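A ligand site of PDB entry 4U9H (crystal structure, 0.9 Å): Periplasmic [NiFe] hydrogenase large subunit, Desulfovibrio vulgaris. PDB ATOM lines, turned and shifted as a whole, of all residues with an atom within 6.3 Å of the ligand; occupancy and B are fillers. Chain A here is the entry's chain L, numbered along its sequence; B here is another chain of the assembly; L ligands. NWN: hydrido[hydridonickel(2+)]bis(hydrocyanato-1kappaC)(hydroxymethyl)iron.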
ATOM      1  N   GLU A  15      14.214  13.519  20.245  1.00  0.00           N
ATOM      2  CA  GLU A  15      12.987  12.792  19.956  1.00  0.00           C
ATOM      3  C   GLU A  15      11.855  13.450  20.758  1.00  0.00           C
ATOM      4  O   GLU A  15      11.979  13.649  21.968  1.00  0.00           O
ATOM      5  CB  GLU A  15      13.133  11.318  20.325  1.00  0.00           C
ATOM      6  CG  GLU A  15      11.992  10.453  19.843  1.00  0.00           C
ATOM      7  CD  GLU A  15      10.685  10.750  20.495  1.00  0.00           C
ATOM      8  OE1 GLU A  15       9.604  10.696  19.793  1.00  0.00           O
ATOM      9  OE2 GLU A  15      10.621  11.017  21.684  1.00  0.00           O
ATOM     10  N   THR A  61       6.544   2.949  22.195  1.00  0.00           N
ATOM     11  CA  THR A  61       6.909   4.098  23.003  1.00  0.00           C
ATOM     12  C   THR A  61       7.871   4.976  22.229  1.00  0.00           C
ATOM     13  O   THR A  61       7.808   6.217  22.332  1.00  0.00           O
ATOM     14  CB  THR A  61       7.548   3.631  24.339  1.00  0.00           C
ATOM     15  OG1 THR A  61       6.575   2.923  25.089  1.00  0.00           O
ATOM     16  CG2 THR A  61       8.038   4.805  25.135  1.00  0.00           C
ATOM     17  N   CYS A  62       8.813   4.376  21.509  1.00  0.00           N
ATOM     18  CA  CYS A  62       9.902   5.151  20.884  1.00  0.00           C
ATOM     19  C   CYS A  62      10.542   4.335  19.779  1.00  0.00           C
ATOM     20  O   CYS A  62      10.921   3.181  19.974  1.00  0.00           O
ATOM     21  CB  CYS A  62      10.936   5.490  21.932  1.00  0.00           C
ATOM     22  SG  CYS A  62      12.203   6.631  21.283  1.00  0.00           S
ATOM     23  N   GLY A  63      10.700   5.003  18.625  1.00  0.00           N
ATOM     24  CA  GLY A  63      11.394   4.423  17.483  1.00  0.00           C
ATOM     25  C   GLY A  63      12.834   4.897  17.300  1.00  0.00           C
ATOM     26  O   GLY A  63      13.489   4.408  16.385  1.00  0.00           O
ATOM     27  N   VAL A  64      13.282   5.839  18.139  1.00  0.00           N
ATOM     28  CA  VAL A  64      14.686   6.200  18.230  1.00  0.00           C
ATOM     29  C   VAL A  64      15.387   5.129  19.063  1.00  0.00           C
ATOM     30  O   VAL A  64      16.238   4.384  18.546  1.00  0.00           O
ATOM     31  CB  VAL A  64      14.883   7.639  18.756  1.00  0.00           C
ATOM     32  CG1 VAL A  64      16.367   7.897  18.940  1.00  0.00           C
ATOM     33  CG2 VAL A  64      14.253   8.624  17.803  1.00  0.00           C
ATOM     34  N   CYS A  65      14.966   4.975  20.322  1.00  0.00           N
ATOM     35  CA  CYS A  65      15.367   3.847  21.150  1.00  0.00           C
ATOM     36  C   CYS A  65      14.441   2.636  20.845  1.00  0.00           C
ATOM     37  O   CYS A  65      13.870   2.003  21.724  1.00  0.00           O
ATOM     38  CB  CYS A  65      15.465   4.188  22.613  1.00  0.00           C
ATOM     39  SG  CYS A  65      13.891   4.669  23.397  1.00  0.00           S
ATOM     40  N   THR A  66      14.323   2.331  19.550  1.00  0.00           N
ATOM     41  CA  THR A  66      13.618   1.130  19.137  1.00  0.00           C
ATOM     42  C   THR A  66      14.285  -0.078  19.795  1.00  0.00           C
ATOM     43  O   THR A  66      15.405  -0.005  20.302  1.00  0.00           O
ATOM     44  CB  THR A  66      13.578   1.053  17.605  1.00  0.00           C
ATOM     45  OG1 THR A  66      12.689   0.026  17.215  1.00  0.00           O
ATOM     46  CG2 THR A  66      14.925   0.733  16.989  1.00  0.00           C
ATOM     47  N   THR A  68      14.449  -1.300  22.594  1.00  0.00           N
ATOM     48  CA  THR A  68      14.660  -1.248  24.043  1.00  0.00           C
ATOM     49  C   THR A  68      13.404  -1.570  24.836  1.00  0.00           C
ATOM     50  O   THR A  68      13.487  -2.301  25.832  1.00  0.00           O
ATOM     51  CB  THR A  68      15.252   0.091  24.488  1.00  0.00           C
ATOM     52  OG1 THR A  68      14.334   1.147  24.384  1.00  0.00           O
ATOM     53  CG2 THR A  68      16.563   0.397  23.782  1.00  0.00           C
ATOM     54  N   HIS A  69      12.242  -1.042  24.438  1.00  0.00           N
ATOM     55  CA  HIS A  69      11.032  -1.295  25.186  1.00  0.00           C
ATOM     56  C   HIS A  69      10.470  -2.685  24.930  1.00  0.00           C
ATOM     57  O   HIS A  69       9.843  -3.280  25.820  1.00  0.00           O
ATOM     58  CB  HIS A  69       9.974  -0.232  24.885  1.00  0.00           C
ATOM     59  CG  HIS A  69      10.291   1.107  25.464  1.00  0.00           C
ATOM     60  ND1 HIS A  69      10.009   1.432  26.780  1.00  0.00           N
ATOM     61  CD2 HIS A  69      10.885   2.167  24.870  1.00  0.00           C
ATOM     62  CE1 HIS A  69      10.422   2.674  26.932  1.00  0.00           C
ATOM     63  NE2 HIS A  69      10.957   3.143  25.811  1.00  0.00           N
ATOM     64  N   ASP A 104      22.397   4.430  17.927  1.00  0.00           N
ATOM     65  CA  ASP A 104      21.727   5.546  18.610  1.00  0.00           C
ATOM     66  C   ASP A 104      22.768   6.623  18.929  1.00  0.00           C
ATOM     67  O   ASP A 104      22.571   7.801  18.632  1.00  0.00           O
ATOM     68  CB  ASP A 104      21.010   4.960  19.830  1.00  0.00           C
ATOM     69  CG  ASP A 104      19.894   5.803  20.408  1.00  0.00           C
ATOM     70  OD1 ASP A 104      19.958   7.060  20.262  1.00  0.00           O
ATOM     71  OD2 ASP A 104      18.999   5.216  21.059  1.00  0.00           O
ATOM     72  N   ALA A 458      19.171   1.372  28.716  1.00  0.00           N
ATOM     73  CA  ALA A 458      19.033   1.797  27.350  1.00  0.00           C
ATOM     74  C   ALA A 458      20.067   2.883  27.034  1.00  0.00           C
ATOM     75  O   ALA A 458      20.759   3.352  27.945  1.00  0.00           O
ATOM     76  CB  ALA A 458      17.611   2.324  27.141  1.00  0.00           C
ATOM     77  N   PRO A 459      20.154   3.351  25.780  1.00  0.00           N
ATOM     78  CA  PRO A 459      21.116   4.425  25.473  1.00  0.00           C
ATOM     79  C   PRO A 459      20.952   5.692  26.325  1.00  0.00           C
ATOM     80  O   PRO A 459      21.928   6.425  26.470  1.00  0.00           O
ATOM     81  CB  PRO A 459      20.897   4.653  23.972  1.00  0.00           C
ATOM     82  CG  PRO A 459      20.495   3.264  23.477  1.00  0.00           C
ATOM     83  CD  PRO A 459      19.548   2.789  24.554  1.00  0.00           C
ATOM     84  N   ARG A 460      19.754   5.956  26.825  1.00  0.00           N
ATOM     85  CA  ARG A 460      19.513   7.121  27.667  1.00  0.00           C
ATOM     86  C   ARG A 460      19.447   6.789  29.161  1.00  0.00           C
ATOM     87  O   ARG A 460      19.265   7.708  29.970  1.00  0.00           O
ATOM     88  CB  ARG A 460      18.269   7.880  27.199  1.00  0.00           C
ATOM     89  CG  ARG A 460      18.492   8.449  25.801  1.00  0.00           C
ATOM     90  CD  ARG A 460      17.196   8.798  25.083  1.00  0.00           C
ATOM     91  NE  ARG A 460      17.425   9.225  23.718  1.00  0.00           N
ATOM     92  CZ  ARG A 460      17.834   8.400  22.724  1.00  0.00           C
ATOM     93  NH1 ARG A 460      17.751   7.081  22.864  1.00  0.00           N
ATOM     94  NH2 ARG A 460      18.265   8.912  21.589  1.00  0.00           N
ATOM     95  N   GLY A 461      19.593   5.522  29.529  1.00  0.00           N
ATOM     96  CA  GLY A 461      19.730   5.130  30.914  1.00  0.00           C
ATOM     97  C   GLY A 461      18.745   4.088  31.380  1.00  0.00           C
ATOM     98  O   GLY A 461      18.286   3.224  30.620  1.00  0.00           O
ATOM     99  N   GLY A 462      18.426   4.131  32.670  1.00  0.00           N
ATOM    100  CA  GLY A 462      17.737   3.023  33.313  1.00  0.00           C
ATOM    101  C   GLY A 462      16.242   2.996  33.009  1.00  0.00           C
ATOM    102  O   GLY A 462      15.459   3.863  33.429  1.00  0.00           O
ATOM    103  N   LEU A 463      15.841   1.966  32.253  1.00  0.00           N
ATOM    104  CA  LEU A 463      14.480   1.697  31.813  1.00  0.00           C
ATOM    105  C   LEU A 463      13.908   0.520  32.626  1.00  0.00           C
ATOM    106  O   LEU A 463      14.546  -0.526  32.738  1.00  0.00           O
ATOM    107  CB  LEU A 463      14.485   1.323  30.321  1.00  0.00           C
ATOM    108  CG  LEU A 463      13.183   0.806  29.740  1.00  0.00           C
ATOM    109  CD1 LEU A 463      12.060   1.824  29.877  1.00  0.00           C
ATOM    110  CD2 LEU A 463      13.363   0.406  28.285  1.00  0.00           C
ATOM    111  N   VAL A 481      10.842   5.497  32.511  1.00  0.00           N
ATOM    112  CA  VAL A 481      11.748   5.497  31.352  1.00  0.00           C
ATOM    113  C   VAL A 481      12.914   6.449  31.640  1.00  0.00           C
ATOM    114  O   VAL A 481      12.764   7.379  32.443  1.00  0.00           O
ATOM    115  CB  VAL A 481      10.893   5.840  30.105  1.00  0.00           C
ATOM    116  CG1 VAL A 481      11.659   5.723  28.798  1.00  0.00           C
ATOM    117  CG2 VAL A 481       9.693   4.887  30.024  1.00  0.00           C
ATOM    118  N   PRO A 482      14.081   6.268  31.005  1.00  0.00           N
ATOM    119  CA  PRO A 482      15.230   7.105  31.416  1.00  0.00           C
ATOM    120  C   PRO A 482      14.954   8.595  31.314  1.00  0.00           C
ATOM    121  O   PRO A 482      15.261   9.357  32.236  1.00  0.00           O
ATOM    122  CB  PRO A 482      16.350   6.631  30.473  1.00  0.00           C
ATOM    123  CG  PRO A 482      15.853   5.417  29.811  1.00  0.00           C
ATOM    124  CD  PRO A 482      14.521   5.121  30.191  1.00  0.00           C
ATOM    125  N   SER A 483      14.357   9.039  30.195  1.00  0.00           N
ATOM    126  CA  SER A 483      14.085  10.464  30.058  1.00  0.00           C
ATOM    127  C   SER A 483      13.051  10.941  31.078  1.00  0.00           C
ATOM    128  O   SER A 483      12.995  12.135  31.363  1.00  0.00           O
ATOM    129  CB  SER A 483      13.639  10.830  28.664  1.00  0.00           C
ATOM    130  OG  SER A 483      14.684  10.690  27.709  1.00  0.00           O
ATOM    131  N   THR A 484      12.216  10.039  31.614  1.00  0.00           N
ATOM    132  CA  THR A 484      11.330  10.429  32.705  1.00  0.00           C
ATOM    133  C   THR A 484      12.163  10.864  33.926  1.00  0.00           C
ATOM    134  O   THR A 484      11.905  11.919  34.536  1.00  0.00           O
ATOM    135  CB  THR A 484      10.361   9.278  33.121  1.00  0.00           C
ATOM    136  OG1 THR A 484       9.929   8.506  31.993  1.00  0.00           O
ATOM    137  CG2 THR A 484       9.180   9.841  33.863  1.00  0.00           C
ATOM    138  N   ASP A 525      20.392  13.898  25.773  1.00  0.00           N
ATOM    139  CA  ASP A 525      19.750  13.109  24.718  1.00  0.00           C
ATOM    140  C   ASP A 525      18.278  12.859  25.034  1.00  0.00           C
ATOM    141  O   ASP A 525      17.838  11.725  25.216  1.00  0.00           O
ATOM    142  CB  ASP A 525      20.559  11.824  24.533  1.00  0.00           C
ATOM    143  CG  ASP A 525      20.171  10.918  23.385  1.00  0.00           C
ATOM    144  OD1 ASP A 525      19.353  11.313  22.531  1.00  0.00           O
ATOM    145  OD2 ASP A 525      20.728   9.785  23.395  1.00  0.00           O
ATOM    146  N   PRO A 526      17.484  13.934  25.131  1.00  0.00           N
ATOM    147  CA  PRO A 526      16.080  13.760  25.512  1.00  0.00           C
ATOM    148  C   PRO A 526      15.270  12.936  24.537  1.00  0.00           C
ATOM    149  O   PRO A 526      15.385  13.058  23.319  1.00  0.00           O
ATOM    150  CB  PRO A 526      15.538  15.212  25.515  1.00  0.00           C
ATOM    151  CG  PRO A 526      16.767  16.070  25.690  1.00  0.00           C
ATOM    152  CD  PRO A 526      17.820  15.351  24.891  1.00  0.00           C
ATOM    153  N   CYS A 527      14.332  12.162  25.107  1.00  0.00           N
ATOM    154  CA  CYS A 527      13.414  11.352  24.332  1.00  0.00           C
ATOM    155  C   CYS A 527      12.057  11.473  24.984  1.00  0.00           C
ATOM    156  O   CYS A 527      11.793  10.878  26.036  1.00  0.00           O
ATOM    157  CB  CYS A 527      13.932   9.927  24.237  1.00  0.00           C
ATOM    158  SG  CYS A 527      13.009   8.948  23.042  1.00  0.00           S
ATOM    159  N   ILE A 528      11.199  12.348  24.432  1.00  0.00           N
ATOM    160  CA  ILE A 528       9.981  12.741  25.142  1.00  0.00           C
ATOM    161  C   ILE A 528       8.857  11.738  24.942  1.00  0.00           C
ATOM    162  O   ILE A 528       8.004  11.571  25.841  1.00  0.00           O
ATOM    163  CB  ILE A 528       9.530  14.172  24.712  1.00  0.00           C
ATOM    164  CG1 ILE A 528      10.718  15.154  24.744  1.00  0.00           C
ATOM    165  CG2 ILE A 528       8.385  14.640  25.606  1.00  0.00           C
ATOM    166  CD1 ILE A 528      11.471  15.256  26.056  1.00  0.00           C
ATOM    167  N   ALA A 529       8.819  11.064  23.800  1.00  0.00           N
ATOM    168  CA  ALA A 529       7.867   9.936  23.625  1.00  0.00           C
ATOM    169  C   ALA A 529       8.191   8.871  24.673  1.00  0.00           C
ATOM    170  O   ALA A 529       7.294   8.319  25.304  1.00  0.00           O
ATOM    171  CB  ALA A 529       7.931   9.423  22.205  1.00  0.00           C
ATOM    172  N   CYS A 530       9.477   8.592  24.867  1.00  0.00           N
ATOM    173  CA  CYS A 530       9.925   7.741  25.976  1.00  0.00           C
ATOM    174  C   CYS A 530       9.487   8.293  27.323  1.00  0.00           C
ATOM    175  O   CYS A 530       8.922   7.562  28.148  1.00  0.00           O
ATOM    176  CB  CYS A 530      11.456   7.627  25.986  1.00  0.00           C
ATOM    177  SG  CYS A 530      11.990   6.122  25.119  1.00  0.00           S
ATOM    178  N   GLY A 531       9.763   9.555  27.609  1.00  0.00           N
ATOM    179  CA  GLY A 531       9.558  10.038  28.951  1.00  0.00           C
ATOM    180  C   GLY A 531       8.095  10.007  29.366  1.00  0.00           C
ATOM    181  O   GLY A 531       7.815   9.787  30.554  1.00  0.00           O
ATOM    182  N   CYS B  15       6.128   8.172  17.646  1.00  0.00           N
ATOM    183  CA  CYS B  15       7.250   7.614  18.343  1.00  0.00           C
ATOM    184  C   CYS B  15       8.583   7.913  17.682  1.00  0.00           C
ATOM    185  O   CYS B  15       9.645   7.546  18.214  1.00  0.00           O
ATOM    186  CB  CYS B  15       7.103   6.098  18.549  1.00  0.00           C
ATOM    187  SG  CYS B  15       7.541   5.114  17.068  1.00  0.00           S
HETATM  188 FE   NWN L   1      14.270   5.752  25.343  1.00  0.00          FE
HETATM  189 NI   NWN L   1      13.441   6.816  23.152  1.00  0.00          NI
HETATM  190  C1  NWN L   1      14.423   7.098  26.643  1.00  0.00           C
HETATM  191  N1  NWN L   1      14.503   7.945  27.438  1.00  0.00           N
HETATM  192  C2  NWN L   1      16.148   5.454  25.315  1.00  0.00           C
HETATM  193  N2  NWN L   1      17.277   5.235  25.348  1.00  0.00           N
HETATM  194  C3  NWN L   1      14.142   4.443  26.501  1.00  0.00           C
HETATM  195  O3  NWN L   1      14.087   3.604  27.283  1.00  0.00           O
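SG of Cys 527 sits close to OE2 of Glu 15 of chain A, at 3.4 Å. O of Cys 65 is in hydrogen-bond range of OG1 of Thr 68, 2.8 Å away. SG of Cys 530 lies close to NE2 of His 69, 3.2 Å away. OG of Ser 483 sits at hydrogen-bond distance from N of Cys 527. N of Val 64 lies close to SG of Cys 62 (3.4 Å). The guanidinium group of Arg 460 lies within salt-bridge range of the side-chain carboxylate of Asp 104, 2.8 Å away. NH2 of Arg 460 lies within salt-bridge range of OD1 of Asp 525, at 2.8 Å. OG1 of Thr 484 lies within hydrogen-bond range of O of Val 481.
N of Pro 459 lies close to N2 of the ligand. Thr 68 touches the ligand (OG1 to O3, 3.8 Å). CB of Ala 458 touches N2 of the ligand, at 3.4 Å. Leu 463 touches the ligand. Val 481 touches the ligand. CD of Pro 482 touches O3 of the ligand (3.3 Å). Of the 28 residues printed, 13 come within 4 Å of the ligand.
An iron atom (FE) of the ligand is bound by the side-chain sulfur (SG) of Cys 530 (2.3 Å). A nickel atom (NI) of the ligand is bound by the side-chain sulfur (SG) of Cys 62, at 2.2 Å. The guanidinium group (NH1) of Arg 460 is in hydrogen-bond range of a nitrogen (N2) of the ligand (3.1 Å). A ring nitrogen (NE2) of His 69 is in hydrogen-bond range of an oxygen (O3) of the ligand. OG of Ser 483 is in hydrogen-bond range of N1 of the ligand (2.8 Å). N of Arg 460 sits at hydrogen-bond distance from N2 of the ligand, 3.0 Å away. NI of the ligand is bound by SG of Cys 527, at 2.2 Å. The side-chain sulfur (SG) of Cys 65 is bound to a nickel atom (NI) of the ligand, 2.2 Å away. N of Ser 483 is in hydrogen-bond range of N1 of the ligand, at 3.0 Å.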
